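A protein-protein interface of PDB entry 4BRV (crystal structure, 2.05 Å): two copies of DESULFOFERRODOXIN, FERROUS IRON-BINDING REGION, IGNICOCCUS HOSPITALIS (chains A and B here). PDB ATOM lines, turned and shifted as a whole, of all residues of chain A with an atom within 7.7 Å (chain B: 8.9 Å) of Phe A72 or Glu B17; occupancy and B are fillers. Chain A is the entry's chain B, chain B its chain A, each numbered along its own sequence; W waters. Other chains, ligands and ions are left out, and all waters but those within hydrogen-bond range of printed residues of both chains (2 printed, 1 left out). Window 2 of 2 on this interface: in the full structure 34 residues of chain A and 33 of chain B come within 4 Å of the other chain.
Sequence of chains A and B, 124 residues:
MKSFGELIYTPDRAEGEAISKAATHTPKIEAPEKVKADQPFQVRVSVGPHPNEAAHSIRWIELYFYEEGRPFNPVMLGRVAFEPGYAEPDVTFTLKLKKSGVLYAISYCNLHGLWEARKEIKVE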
ATOM      1  N   PHE A  65      -1.132 -16.019  10.015  1.00  0.00           N
ATOM      2  CA  PHE A  65      -0.549 -16.488  11.267  1.00  0.00           C
ATOM      3  C   PHE A  65      -0.934 -15.541  12.388  1.00  0.00           C
ATOM      4  O   PHE A  65      -0.685 -14.331  12.295  1.00  0.00           O
ATOM      5  CB  PHE A  65       0.978 -16.493  11.159  1.00  0.00           C
ATOM      6  CG  PHE A  65       1.677 -17.239  12.272  1.00  0.00           C
ATOM      7  CD1 PHE A  65       1.610 -18.617  12.352  1.00  0.00           C
ATOM      8  CD2 PHE A  65       2.427 -16.557  13.220  1.00  0.00           C
ATOM      9  CE1 PHE A  65       2.276 -19.303  13.369  1.00  0.00           C
ATOM     10  CE2 PHE A  65       3.103 -17.239  14.229  1.00  0.00           C
ATOM     11  CZ  PHE A  65       3.021 -18.596  14.308  1.00  0.00           C
ATOM     12  N   TYR A  66      -1.545 -16.073  13.440  1.00  0.00           N
ATOM     13  CA  TYR A  66      -1.720 -15.303  14.668  1.00  0.00           C
ATOM     14  C   TYR A  66      -0.419 -15.439  15.449  1.00  0.00           C
ATOM     15  O   TYR A  66      -0.040 -16.548  15.869  1.00  0.00           O
ATOM     16  CB  TYR A  66      -2.864 -15.883  15.495  1.00  0.00           C
ATOM     17  CG  TYR A  66      -3.117 -15.148  16.785  1.00  0.00           C
ATOM     18  CD1 TYR A  66      -2.459 -15.496  17.946  1.00  0.00           C
ATOM     19  CD2 TYR A  66      -4.010 -14.085  16.829  1.00  0.00           C
ATOM     20  CE1 TYR A  66      -2.696 -14.818  19.120  1.00  0.00           C
ATOM     21  CE2 TYR A  66      -4.255 -13.407  17.986  1.00  0.00           C
ATOM     22  CZ  TYR A  66      -3.597 -13.774  19.131  1.00  0.00           C
ATOM     23  OH  TYR A  66      -3.842 -13.086  20.295  1.00  0.00           O
ATOM     24  N   GLU A  67       0.284 -14.333  15.633  1.00  0.00           N
ATOM     25  CA  GLU A  67       1.584 -14.401  16.284  1.00  0.00           C
ATOM     26  C   GLU A  67       1.477 -13.948  17.731  1.00  0.00           C
ATOM     27  O   GLU A  67       0.999 -12.840  18.018  1.00  0.00           O
ATOM     28  CB  GLU A  67       2.583 -13.536  15.527  1.00  0.00           C
ATOM     29  CG  GLU A  67       3.972 -13.538  16.119  1.00  0.00           C
ATOM     30  CD  GLU A  67       4.922 -12.732  15.266  1.00  0.00           C
ATOM     31  OE1 GLU A  67       5.370 -13.256  14.220  1.00  0.00           O
ATOM     32  OE2 GLU A  67       5.190 -11.563  15.619  1.00  0.00           O
ATOM     33  N   GLY A  69       1.760 -12.436  21.301  1.00  0.00           N
ATOM     34  CA  GLY A  69       2.334 -11.189  21.777  1.00  0.00           C
ATOM     35  C   GLY A  69       2.277 -10.007  20.812  1.00  0.00           C
ATOM     36  O   GLY A  69       2.662  -8.907  21.189  1.00  0.00           O
ATOM     37  N   ARG A  70       1.825 -10.204  19.575  1.00  0.00           N
ATOM     38  CA  ARG A  70       1.787  -9.076  18.626  1.00  0.00           C
ATOM     39  C   ARG A  70       0.664  -8.104  18.995  1.00  0.00           C
ATOM     40  O   ARG A  70      -0.436  -8.542  19.331  1.00  0.00           O
ATOM     41  CB  ARG A  70       1.597  -9.584  17.194  1.00  0.00           C
ATOM     42  CG  ARG A  70       2.194  -8.679  16.102  1.00  0.00           C
ATOM     43  CD  ARG A  70       2.113  -9.378  14.755  1.00  0.00           C
ATOM     44  NE  ARG A  70       2.686  -8.611  13.638  1.00  0.00           N
ATOM     45  CZ  ARG A  70       1.954  -7.950  12.737  1.00  0.00           C
ATOM     46  NH1 ARG A  70       0.628  -7.931  12.837  1.00  0.00           N
ATOM     47  NH2 ARG A  70       2.534  -7.317  11.728  1.00  0.00           N
ATOM     48  N   PRO A  71       0.931  -6.782  18.937  1.00  0.00           N
ATOM     49  CA  PRO A  71      -0.118  -5.836  19.325  1.00  0.00           C
ATOM     50  C   PRO A  71      -1.349  -5.996  18.452  1.00  0.00           C
ATOM     51  O   PRO A  71      -2.457  -5.801  18.949  1.00  0.00           O
ATOM     52  CB  PRO A  71       0.521  -4.467  19.051  1.00  0.00           C
ATOM     53  CG  PRO A  71       1.972  -4.708  19.035  1.00  0.00           C
ATOM     54  CD  PRO A  71       2.133  -6.079  18.454  1.00  0.00           C
ATOM     55  N   PHE A  72      -1.163  -6.359  17.185  1.00  0.00           N
ATOM     56  CA  PHE A  72      -2.299  -6.605  16.290  1.00  0.00           C
ATOM     57  C   PHE A  72      -2.052  -7.897  15.545  1.00  0.00           C
ATOM     58  O   PHE A  72      -0.907  -8.331  15.434  1.00  0.00           O
ATOM     59  CB  PHE A  72      -2.456  -5.472  15.274  1.00  0.00           C
ATOM     60  CG  PHE A  72      -2.722  -4.121  15.893  1.00  0.00           C
ATOM     61  CD1 PHE A  72      -1.684  -3.359  16.404  1.00  0.00           C
ATOM     62  CD2 PHE A  72      -4.014  -3.605  15.938  1.00  0.00           C
ATOM     63  CE1 PHE A  72      -1.922  -2.103  16.962  1.00  0.00           C
ATOM     64  CE2 PHE A  72      -4.262  -2.343  16.500  1.00  0.00           C
ATOM     65  CZ  PHE A  72      -3.215  -1.599  17.013  1.00  0.00           C
ATOM     66  N   ASN A  73      -3.124  -8.501  15.029  1.00  0.00           N
ATOM     67  CA  ASN A  73      -3.042  -9.807  14.396  1.00  0.00           C
ATOM     68  C   ASN A  73      -4.218  -9.905  13.443  1.00  0.00           C
ATOM     69  O   ASN A  73      -5.183  -9.145  13.589  1.00  0.00           O
ATOM     70  CB  ASN A  73      -3.112 -10.909  15.462  1.00  0.00           C
ATOM     71  CG  ASN A  73      -1.726 -11.459  15.849  1.00  0.00           C
ATOM     72  OD1 ASN A  73      -0.921 -11.830  14.986  1.00  0.00           O
ATOM     73  ND2 ASN A  73      -1.458 -11.525  17.148  1.00  0.00           N
ATOM     74  N   PRO A  74      -4.146 -10.819  12.463  1.00  0.00           N
ATOM     75  CA  PRO A  74      -2.984 -11.686  12.216  1.00  0.00           C
ATOM     76  C   PRO A  74      -2.045 -11.089  11.177  1.00  0.00           C
ATOM     77  O   PRO A  74      -2.285  -9.984  10.633  1.00  0.00           O
ATOM     78  CB  PRO A  74      -3.626 -12.948  11.638  1.00  0.00           C
ATOM     79  CG  PRO A  74      -4.794 -12.380  10.800  1.00  0.00           C
ATOM     80  CD  PRO A  74      -5.253 -11.109  11.528  1.00  0.00           C
ATOM     81  N   VAL A  75      -0.974 -11.830  10.916  1.00  0.00           N
ATOM     82  CA  VAL A  75      -0.025 -11.510   9.862  1.00  0.00           C
ATOM     83  C   VAL A  75      -0.357 -12.389   8.679  1.00  0.00           C
ATOM     84  O   VAL A  75      -0.452 -13.605   8.822  1.00  0.00           O
ATOM     85  CB  VAL A  75       1.418 -11.862  10.282  1.00  0.00           C
ATOM     86  CG1 VAL A  75       2.382 -11.475   9.171  1.00  0.00           C
ATOM     87  CG2 VAL A  75       1.779 -11.156  11.566  1.00  0.00           C
ATOM     88  N   LEU B   7     -10.827 -12.552  14.450  1.00  0.00           N
ATOM     89  CA  LEU B   7      -9.638 -11.711  14.450  1.00  0.00           C
ATOM     90  C   LEU B   7      -9.849 -10.414  13.684  1.00  0.00           C
ATOM     91  O   LEU B   7      -9.146  -9.425  13.915  1.00  0.00           O
ATOM     92  CB  LEU B   7      -8.454 -12.468  13.840  1.00  0.00           C
ATOM     93  CG  LEU B   7      -8.019 -13.759  14.530  1.00  0.00           C
ATOM     94  CD1 LEU B   7      -6.756 -14.266  13.858  1.00  0.00           C
ATOM     95  CD2 LEU B   7      -7.773 -13.524  16.004  1.00  0.00           C
ATOM     96  N   TYR B   9     -10.916  -6.939  12.581  1.00  0.00           N
ATOM     97  CA  TYR B   9     -11.348  -5.741  13.295  1.00  0.00           C
ATOM     98  C   TYR B   9     -12.547  -5.062  12.639  1.00  0.00           C
ATOM     99  O   TYR B   9     -12.594  -4.888  11.420  1.00  0.00           O
ATOM    100  CB  TYR B   9     -10.193  -4.734  13.421  1.00  0.00           C
ATOM    101  CG  TYR B   9      -8.997  -5.287  14.164  1.00  0.00           C
ATOM    102  CD1 TYR B   9      -9.051  -5.498  15.524  1.00  0.00           C
ATOM    103  CD2 TYR B   9      -7.820  -5.595  13.497  1.00  0.00           C
ATOM    104  CE1 TYR B   9      -7.962  -6.019  16.218  1.00  0.00           C
ATOM    105  CE2 TYR B   9      -6.724  -6.107  14.174  1.00  0.00           C
ATOM    106  CZ  TYR B   9      -6.804  -6.325  15.532  1.00  0.00           C
ATOM    107  OH  TYR B   9      -5.715  -6.839  16.200  1.00  0.00           O
ATOM    108  N   ALA B  14     -14.105  -2.927  18.365  1.00  0.00           N
ATOM    109  CA  ALA B  14     -12.723  -2.551  18.682  1.00  0.00           C
ATOM    110  C   ALA B  14     -12.423  -2.582  20.181  1.00  0.00           C
ATOM    111  O   ALA B  14     -13.054  -1.870  20.962  1.00  0.00           O
ATOM    112  CB  ALA B  14     -12.400  -1.173  18.108  1.00  0.00           C
ATOM    113  N   GLU B  15     -11.458  -3.410  20.574  1.00  0.00           N
ATOM    114  CA  GLU B  15     -11.037  -3.489  21.972  1.00  0.00           C
ATOM    115  C   GLU B  15      -9.677  -2.833  22.183  1.00  0.00           C
ATOM    116  O   GLU B  15      -8.732  -3.089  21.433  1.00  0.00           O
ATOM    117  CB  GLU B  15     -10.986  -4.945  22.455  1.00  0.00           C
ATOM    118  CG  GLU B  15     -12.347  -5.615  22.618  1.00  0.00           C
ATOM    119  CD  GLU B  15     -12.482  -6.871  21.777  1.00  0.00           C
ATOM    120  OE1 GLU B  15     -11.469  -7.299  21.182  1.00  0.00           O
ATOM    121  OE2 GLU B  15     -13.600  -7.425  21.706  1.00  0.00           O
ATOM    122  N   GLY B  16      -9.588  -1.985  23.203  1.00  0.00           N
ATOM    123  CA  GLY B  16      -8.324  -1.398  23.617  1.00  0.00           C
ATOM    124  C   GLY B  16      -7.585  -0.569  22.583  1.00  0.00           C
ATOM    125  O   GLY B  16      -8.131   0.388  22.026  1.00  0.00           O
ATOM    126  N   GLU B  17      -6.331  -0.945  22.333  1.00  0.00           N
ATOM    127  CA  GLU B  17      -5.437  -0.197  21.451  1.00  0.00           C
ATOM    128  C   GLU B  17      -5.998  -0.029  20.037  1.00  0.00           C
ATOM    129  O   GLU B  17      -5.685   0.945  19.349  1.00  0.00           O
ATOM    130  CB  GLU B  17      -4.059  -0.872  21.400  1.00  0.00           C
ATOM    131  CG  GLU B  17      -2.954  -0.006  20.806  1.00  0.00           C
ATOM    132  CD  GLU B  17      -1.590  -0.676  20.842  1.00  0.00           C
ATOM    133  OE1 GLU B  17      -1.411  -1.635  21.627  1.00  0.00           O
ATOM    134  OE2 GLU B  17      -0.695  -0.243  20.082  1.00  0.00           O
ATOM    135  N   ALA B  18      -6.837  -0.974  19.616  1.00  0.00           N
ATOM    136  CA  ALA B  18      -7.393  -0.967  18.266  1.00  0.00           C
ATOM    137  C   ALA B  18      -8.461   0.103  18.042  1.00  0.00           C
ATOM    138  O   ALA B  18      -8.745   0.458  16.899  1.00  0.00           O
ATOM    139  CB  ALA B  18      -7.944  -2.345  17.910  1.00  0.00           C
ATOM    140  N   ILE B  19      -9.061   0.601  19.123  1.00  0.00           N
ATOM    141  CA  ILE B  19     -10.088   1.646  19.019  1.00  0.00           C
ATOM    142  C   ILE B  19      -9.535   2.895  18.322  1.00  0.00           C
ATOM    143  O   ILE B  19     -10.184   3.468  17.439  1.00  0.00           O
ATOM    144  CB  ILE B  19     -10.659   2.028  20.406  1.00  0.00           C
ATOM    145  CG1 ILE B  19     -11.461   0.865  20.995  1.00  0.00           C
ATOM    146  CG2 ILE B  19     -11.545   3.255  20.303  1.00  0.00           C
ATOM    147  CD1 ILE B  19     -11.898   1.066  22.436  1.00  0.00           C
ATOM    148  N   SER B  20      -8.320   3.289  18.705  1.00  0.00           N
ATOM    149  CA  SER B  20      -7.662   4.458  18.122  1.00  0.00           C
ATOM    150  C   SER B  20      -7.176   4.292  16.669  1.00  0.00           C
ATOM    151  O   SER B  20      -6.907   5.287  15.998  1.00  0.00           O
ATOM    152  CB  SER B  20      -6.512   4.921  19.021  1.00  0.00           C
ATOM    153  OG  SER B  20      -5.757   3.819  19.495  1.00  0.00           O
ATOM    154  N   LYS B  21      -7.075   3.056  16.180  1.00  0.00           N
ATOM    155  CA  LYS B  21      -6.621   2.807  14.810  1.00  0.00           C
ATOM    156  C   LYS B  21      -7.789   2.717  13.814  1.00  0.00           C
ATOM    157  O   LYS B  21      -7.578   2.664  12.599  1.00  0.00           O
ATOM    158  CB  LYS B  21      -5.796   1.510  14.744  1.00  0.00           C
ATOM    159  CG  LYS B  21      -4.596   1.438  15.683  1.00  0.00           C
ATOM    160  CD  LYS B  21      -3.588   2.557  15.415  1.00  0.00           C
ATOM    161  CE  LYS B  21      -2.780   2.297  14.148  1.00  0.00           C
ATOM    162  NZ  LYS B  21      -2.077   3.505  13.606  1.00  0.00           N
ATOM    163  N   ALA B  22      -9.015   2.705  14.332  1.00  0.00           N
ATOM    164  CA  ALA B  22     -10.191   2.322  13.541  1.00  0.00           C
ATOM    165  C   ALA B  22     -10.544   3.290  12.410  1.00  0.00           C
ATOM    166  O   ALA B  22     -10.875   2.860  11.300  1.00  0.00           O
ATOM    167  CB  ALA B  22     -11.402   2.107  14.452  1.00  0.00           C
ATOM    168  N   HIS B  25      -8.114   2.828   9.421  1.00  0.00           N
ATOM    169  CA  HIS B  25      -7.962   1.520   8.788  1.00  0.00           C
ATOM    170  C   HIS B  25      -9.264   0.949   8.214  1.00  0.00           C
ATOM    171  O   HIS B  25      -9.216   0.172   7.265  1.00  0.00           O
ATOM    172  CB  HIS B  25      -7.321   0.501   9.742  1.00  0.00           C
ATOM    173  CG  HIS B  25      -5.891   0.798  10.076  1.00  0.00           C
ATOM    174  ND1 HIS B  25      -5.531   1.679  11.073  1.00  0.00           N
ATOM    175  CD2 HIS B  25      -4.734   0.336   9.545  1.00  0.00           C
ATOM    176  CE1 HIS B  25      -4.213   1.734  11.153  1.00  0.00           C
ATOM    177  NE2 HIS B  25      -3.704   0.927  10.239  1.00  0.00           N
ATOM    178  N   HIS B  56       5.133   0.038   6.043  1.00  0.00           N
ATOM    179  CA  HIS B  56       3.808   0.253   6.620  1.00  0.00           C
ATOM    180  C   HIS B  56       2.849   0.795   5.566  1.00  0.00           C
ATOM    181  O   HIS B  56       2.940   1.975   5.180  1.00  0.00           O
ATOM    182  CB  HIS B  56       3.904   1.275   7.779  1.00  0.00           C
ATOM    183  CG  HIS B  56       2.612   1.477   8.520  1.00  0.00           C
ATOM    184  ND1 HIS B  56       2.430   2.490   9.438  1.00  0.00           N
ATOM    185  CD2 HIS B  56       1.440   0.793   8.469  1.00  0.00           C
ATOM    186  CE1 HIS B  56       1.201   2.425   9.925  1.00  0.00           C
ATOM    187  NE2 HIS B  56       0.579   1.405   9.352  1.00  0.00           N
ATOM    188  N   TYR B 108      -6.187  -4.693   4.392  1.00  0.00           N
ATOM    189  CA  TYR B 108      -5.118  -5.254   5.214  1.00  0.00           C
ATOM    190  C   TYR B 108      -3.969  -4.270   5.335  1.00  0.00           C
ATOM    191  O   TYR B 108      -3.446  -3.775   4.326  1.00  0.00           O
ATOM    192  CB  TYR B 108      -4.619  -6.586   4.629  1.00  0.00           C
ATOM    193  CG  TYR B 108      -3.391  -7.173   5.325  1.00  0.00           C
ATOM    194  CD1 TYR B 108      -3.519  -7.884   6.508  1.00  0.00           C
ATOM    195  CD2 TYR B 108      -2.112  -7.042   4.776  1.00  0.00           C
ATOM    196  CE1 TYR B 108      -2.397  -8.445   7.159  1.00  0.00           C
ATOM    197  CE2 TYR B 108      -0.974  -7.608   5.411  1.00  0.00           C
ATOM    198  CZ  TYR B 108      -1.138  -8.307   6.603  1.00  0.00           C
ATOM    199  OH  TYR B 108      -0.056  -8.871   7.252  1.00  0.00           O
ATOM    200  N   CYS B 109      -3.600  -3.966   6.579  1.00  0.00           N
ATOM    201  CA  CYS B 109      -2.409  -3.197   6.868  1.00  0.00           C
ATOM    202  C   CYS B 109      -1.351  -4.172   7.409  1.00  0.00           C
ATOM    203  O   CYS B 109      -1.652  -4.960   8.319  1.00  0.00           O
ATOM    204  CB  CYS B 109      -2.735  -2.150   7.933  1.00  0.00           C
ATOM    205  SG  CYS B 109      -1.298  -1.247   8.593  1.00  0.00           S
ATOM    206  N   ASN B 110      -0.122  -4.132   6.887  1.00  0.00           N
ATOM    207  CA  ASN B 110       0.891  -5.121   7.325  1.00  0.00           C
ATOM    208  C   ASN B 110       1.171  -5.082   8.829  1.00  0.00           C
ATOM    209  O   ASN B 110       1.582  -6.078   9.403  1.00  0.00           O
ATOM    210  CB  ASN B 110       2.219  -5.001   6.536  1.00  0.00           C
ATOM    211  CG  ASN B 110       2.896  -3.641   6.719  1.00  0.00           C
ATOM    212  OD1 ASN B 110       2.287  -2.594   6.459  1.00  0.00           O
ATOM    213  ND2 ASN B 110       4.162  -3.650   7.159  1.00  0.00           N
ATOM    214  N   LEU B 111       0.951  -3.930   9.465  1.00  0.00           N
ATOM    215  CA  LEU B 111       1.185  -3.794  10.911  1.00  0.00           C
ATOM    216  C   LEU B 111      -0.080  -3.983  11.744  1.00  0.00           C
ATOM    217  O   LEU B 111      -0.015  -4.437  12.894  1.00  0.00           O
ATOM    218  CB  LEU B 111       1.768  -2.402  11.245  1.00  0.00           C
ATOM    219  CG  LEU B 111       3.186  -2.070  10.782  1.00  0.00           C
ATOM    220  CD1 LEU B 111       3.617  -0.702  11.320  1.00  0.00           C
ATOM    221  CD2 LEU B 111       4.182  -3.168  11.194  1.00  0.00           C
ATOM    222  N   HIS B 112      -1.224  -3.600  11.181  1.00  0.00           N
ATOM    223  CA  HIS B 112      -2.410  -3.379  11.995  1.00  0.00           C
ATOM    224  C   HIS B 112      -3.599  -4.255  11.629  1.00  0.00           C
ATOM    225  O   HIS B 112      -4.722  -4.008  12.092  1.00  0.00           O
ATOM    226  CB  HIS B 112      -2.769  -1.880  11.977  1.00  0.00           C
ATOM    227  CG  HIS B 112      -1.668  -1.010  12.513  1.00  0.00           C
ATOM    228  ND1 HIS B 112      -1.260   0.157  11.898  1.00  0.00           N
ATOM    229  CD2 HIS B 112      -0.864  -1.161  13.594  1.00  0.00           C
ATOM    230  CE1 HIS B 112      -0.258   0.686  12.577  1.00  0.00           C
ATOM    231  NE2 HIS B 112       0.001  -0.093  13.615  1.00  0.00           N
ATOM    232  N   GLY B 113      -3.356  -5.264  10.792  1.00  0.00           N
ATOM    233  CA  GLY B 113      -4.302  -6.357  10.634  1.00  0.00           C
ATOM    234  C   GLY B 113      -5.404  -6.113   9.612  1.00  0.00           C
ATOM    235  O   GLY B 113      -5.257  -5.276   8.708  1.00  0.00           O
ATOM    236  N   LEU B 114      -6.508  -6.846   9.776  1.00  0.00           N
ATOM    237  CA  LEU B 114      -7.604  -6.868   8.813  1.00  0.00           C
ATOM    238  C   LEU B 114      -8.772  -6.061   9.336  1.00  0.00           C
ATOM    239  O   LEU B 114      -9.190  -6.246  10.477  1.00  0.00           O
ATOM    240  CB  LEU B 114      -8.069  -8.314   8.603  1.00  0.00           C
ATOM    241  CG  LEU B 114      -7.082  -9.242   7.915  1.00  0.00           C
ATOM    242  CD1 LEU B 114      -7.428 -10.683   8.219  1.00  0.00           C
ATOM    243  CD2 LEU B 114      -7.182  -8.997   6.434  1.00  0.00           C
ATOM    244  N   TRP B 115      -9.320  -5.183   8.499  1.00  0.00           N
ATOM    245  CA  TRP B 115     -10.432  -4.338   8.919  1.00  0.00           C
ATOM    246  C   TRP B 115     -11.612  -4.475   7.969  1.00  0.00           C
ATOM    247  O   TRP B 115     -11.436  -4.567   6.745  1.00  0.00           O
ATOM    248  CB  TRP B 115      -9.981  -2.883   8.984  1.00  0.00           C
ATOM    249  CG  TRP B 115      -9.030  -2.667  10.124  1.00  0.00           C
ATOM    250  CD1 TRP B 115      -7.700  -2.995  10.163  1.00  0.00           C
ATOM    251  CD2 TRP B 115      -9.349  -2.113  11.405  1.00  0.00           C
ATOM    252  NE1 TRP B 115      -7.172  -2.668  11.403  1.00  0.00           N
ATOM    253  CE2 TRP B 115      -8.167  -2.125  12.177  1.00  0.00           C
ATOM    254  CE3 TRP B 115     -10.521  -1.609  11.974  1.00  0.00           C
ATOM    255  CZ2 TRP B 115      -8.131  -1.650  13.490  1.00  0.00           C
ATOM    256  CZ3 TRP B 115     -10.486  -1.140  13.266  1.00  0.00           C
ATOM    257  CH2 TRP B 115      -9.296  -1.155  14.015  1.00  0.00           C
HETATM  258  O   HOH W   1      -7.152  -8.508  12.005  1.00  0.00           O
HETATM  259  O   HOH W   2      -7.045  -9.717  15.880  1.00  0.00           O
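Water W1 lies within hydrogen-bond range of O of Asn A73 (2.6 Å), N of Leu B114 (2.9 Å) and O of Leu B7 (2.9 Å).
Water W2 lies within hydrogen-bond range of O of Leu B7, O of Asn A73 and OH of Tyr B9.
Among the printed residues, pairs that only touch across the chains: Phe A72 with Tyr B9, Arg A70 with Leu B111, Phe A72 with Leu B111, Phe A72 with Lys B21, Phe A72 with His B112, Val A75 with Tyr B108, Pro A74 with Tyr B108, Phe A72 with Glu B17, Phe A72 with Ala B18, Tyr A66 with Leu B7, Pro A74 with Leu B114 and Asn A73 with Leu B7.
The backbone NH (N) of Glu A67 sits at hydrogen-bond distance from the side-chain amide oxygen (OD1) of Asn A73 (2.9 Å).
The backbone carbonyl oxygen (O) of Phe A72 lies within hydrogen-bond range of the guanidinium group (NH1) of Arg A70, 3.0 Å away.
The backbone NH (N) of Tyr B9 is in hydrogen-bond range of the backbone carbonyl oxygen (O) of Leu B114 (2.8 Å).
The backbone carbonyl oxygen of Lys B21 sits at hydrogen-bond distance from a ring nitrogen (ND1) of His B25 (2.7 Å).
The indole nitrogen of Trp B115 is in hydrogen-bond range of the backbone carbonyl oxygen of His B112, at 2.9 Å.
The backbone NH (N) of Phe A65 sits at hydrogen-bond distance from the backbone carbonyl oxygen (O) of Val A75.
The backbone carbonyl oxygen of Asn B110 sits at hydrogen-bond distance from the guanidinium group of Arg A70 (2.8 Å).
OH of Tyr B9 is in hydrogen-bond range of N of Asn A73 (3.3 Å).
No residue of chain B comes within 4 Å of Pro A71.
Printed residues of chain B within 4 Å of Asn A73: Leu B7 (3.99 Å) and Tyr B9 (3.3 Å).
Of the printed residues of chain B, Val A75 touches Tyr B108 (3.7 Å).
Printed residues of chain A within 4 Å of Tyr B9: Phe A72 (3.4 Å) and Asn A73 (3.3 Å).
Of chain A, only Phe A72 (3.8 Å) comes within 4 Å of Glu B17.
Printed residues of chain A within 4 Å of Leu B111: Arg A70 (3.6 Å) and Phe A72 (3.6 Å).
Printed residues of chain B that touch a printed residue of chain A: Leu B7, Tyr B9, Glu B17, Ala B18, Lys B21, Tyr B108, Asn B110, Leu B111, His B112 and Leu B114.
Hydrophobic or aromatic side chains of chain B that line the printed part of chain A: Leu B7, Tyr B9, Ala B18, Tyr B108, His B112 and Leu B114.
Of the 10 printed residues of chain A, 6 touch a printed residue of chain B.
Printed residues of chain A that touch a printed residue of chain B: Tyr A66, Arg A70, Phe A72, Asn A73, Pro A74 and Val A75.
Hydrophobic or aromatic side chains of chain A that line the printed part of chain B: Tyr A66, Phe A72 and Pro A74.
Among the printed residues, 14 pairs touch across the chains.
Among the printed residues, no Asp or Glu carboxylate lies within 4 Å of a Lys or Arg side-chain nitrogen of the other chain.
No position is printed for both chains.
Of the 14 pairs that touch across the chains among the printed residues, none has its exchanged pair printed and touching as well.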
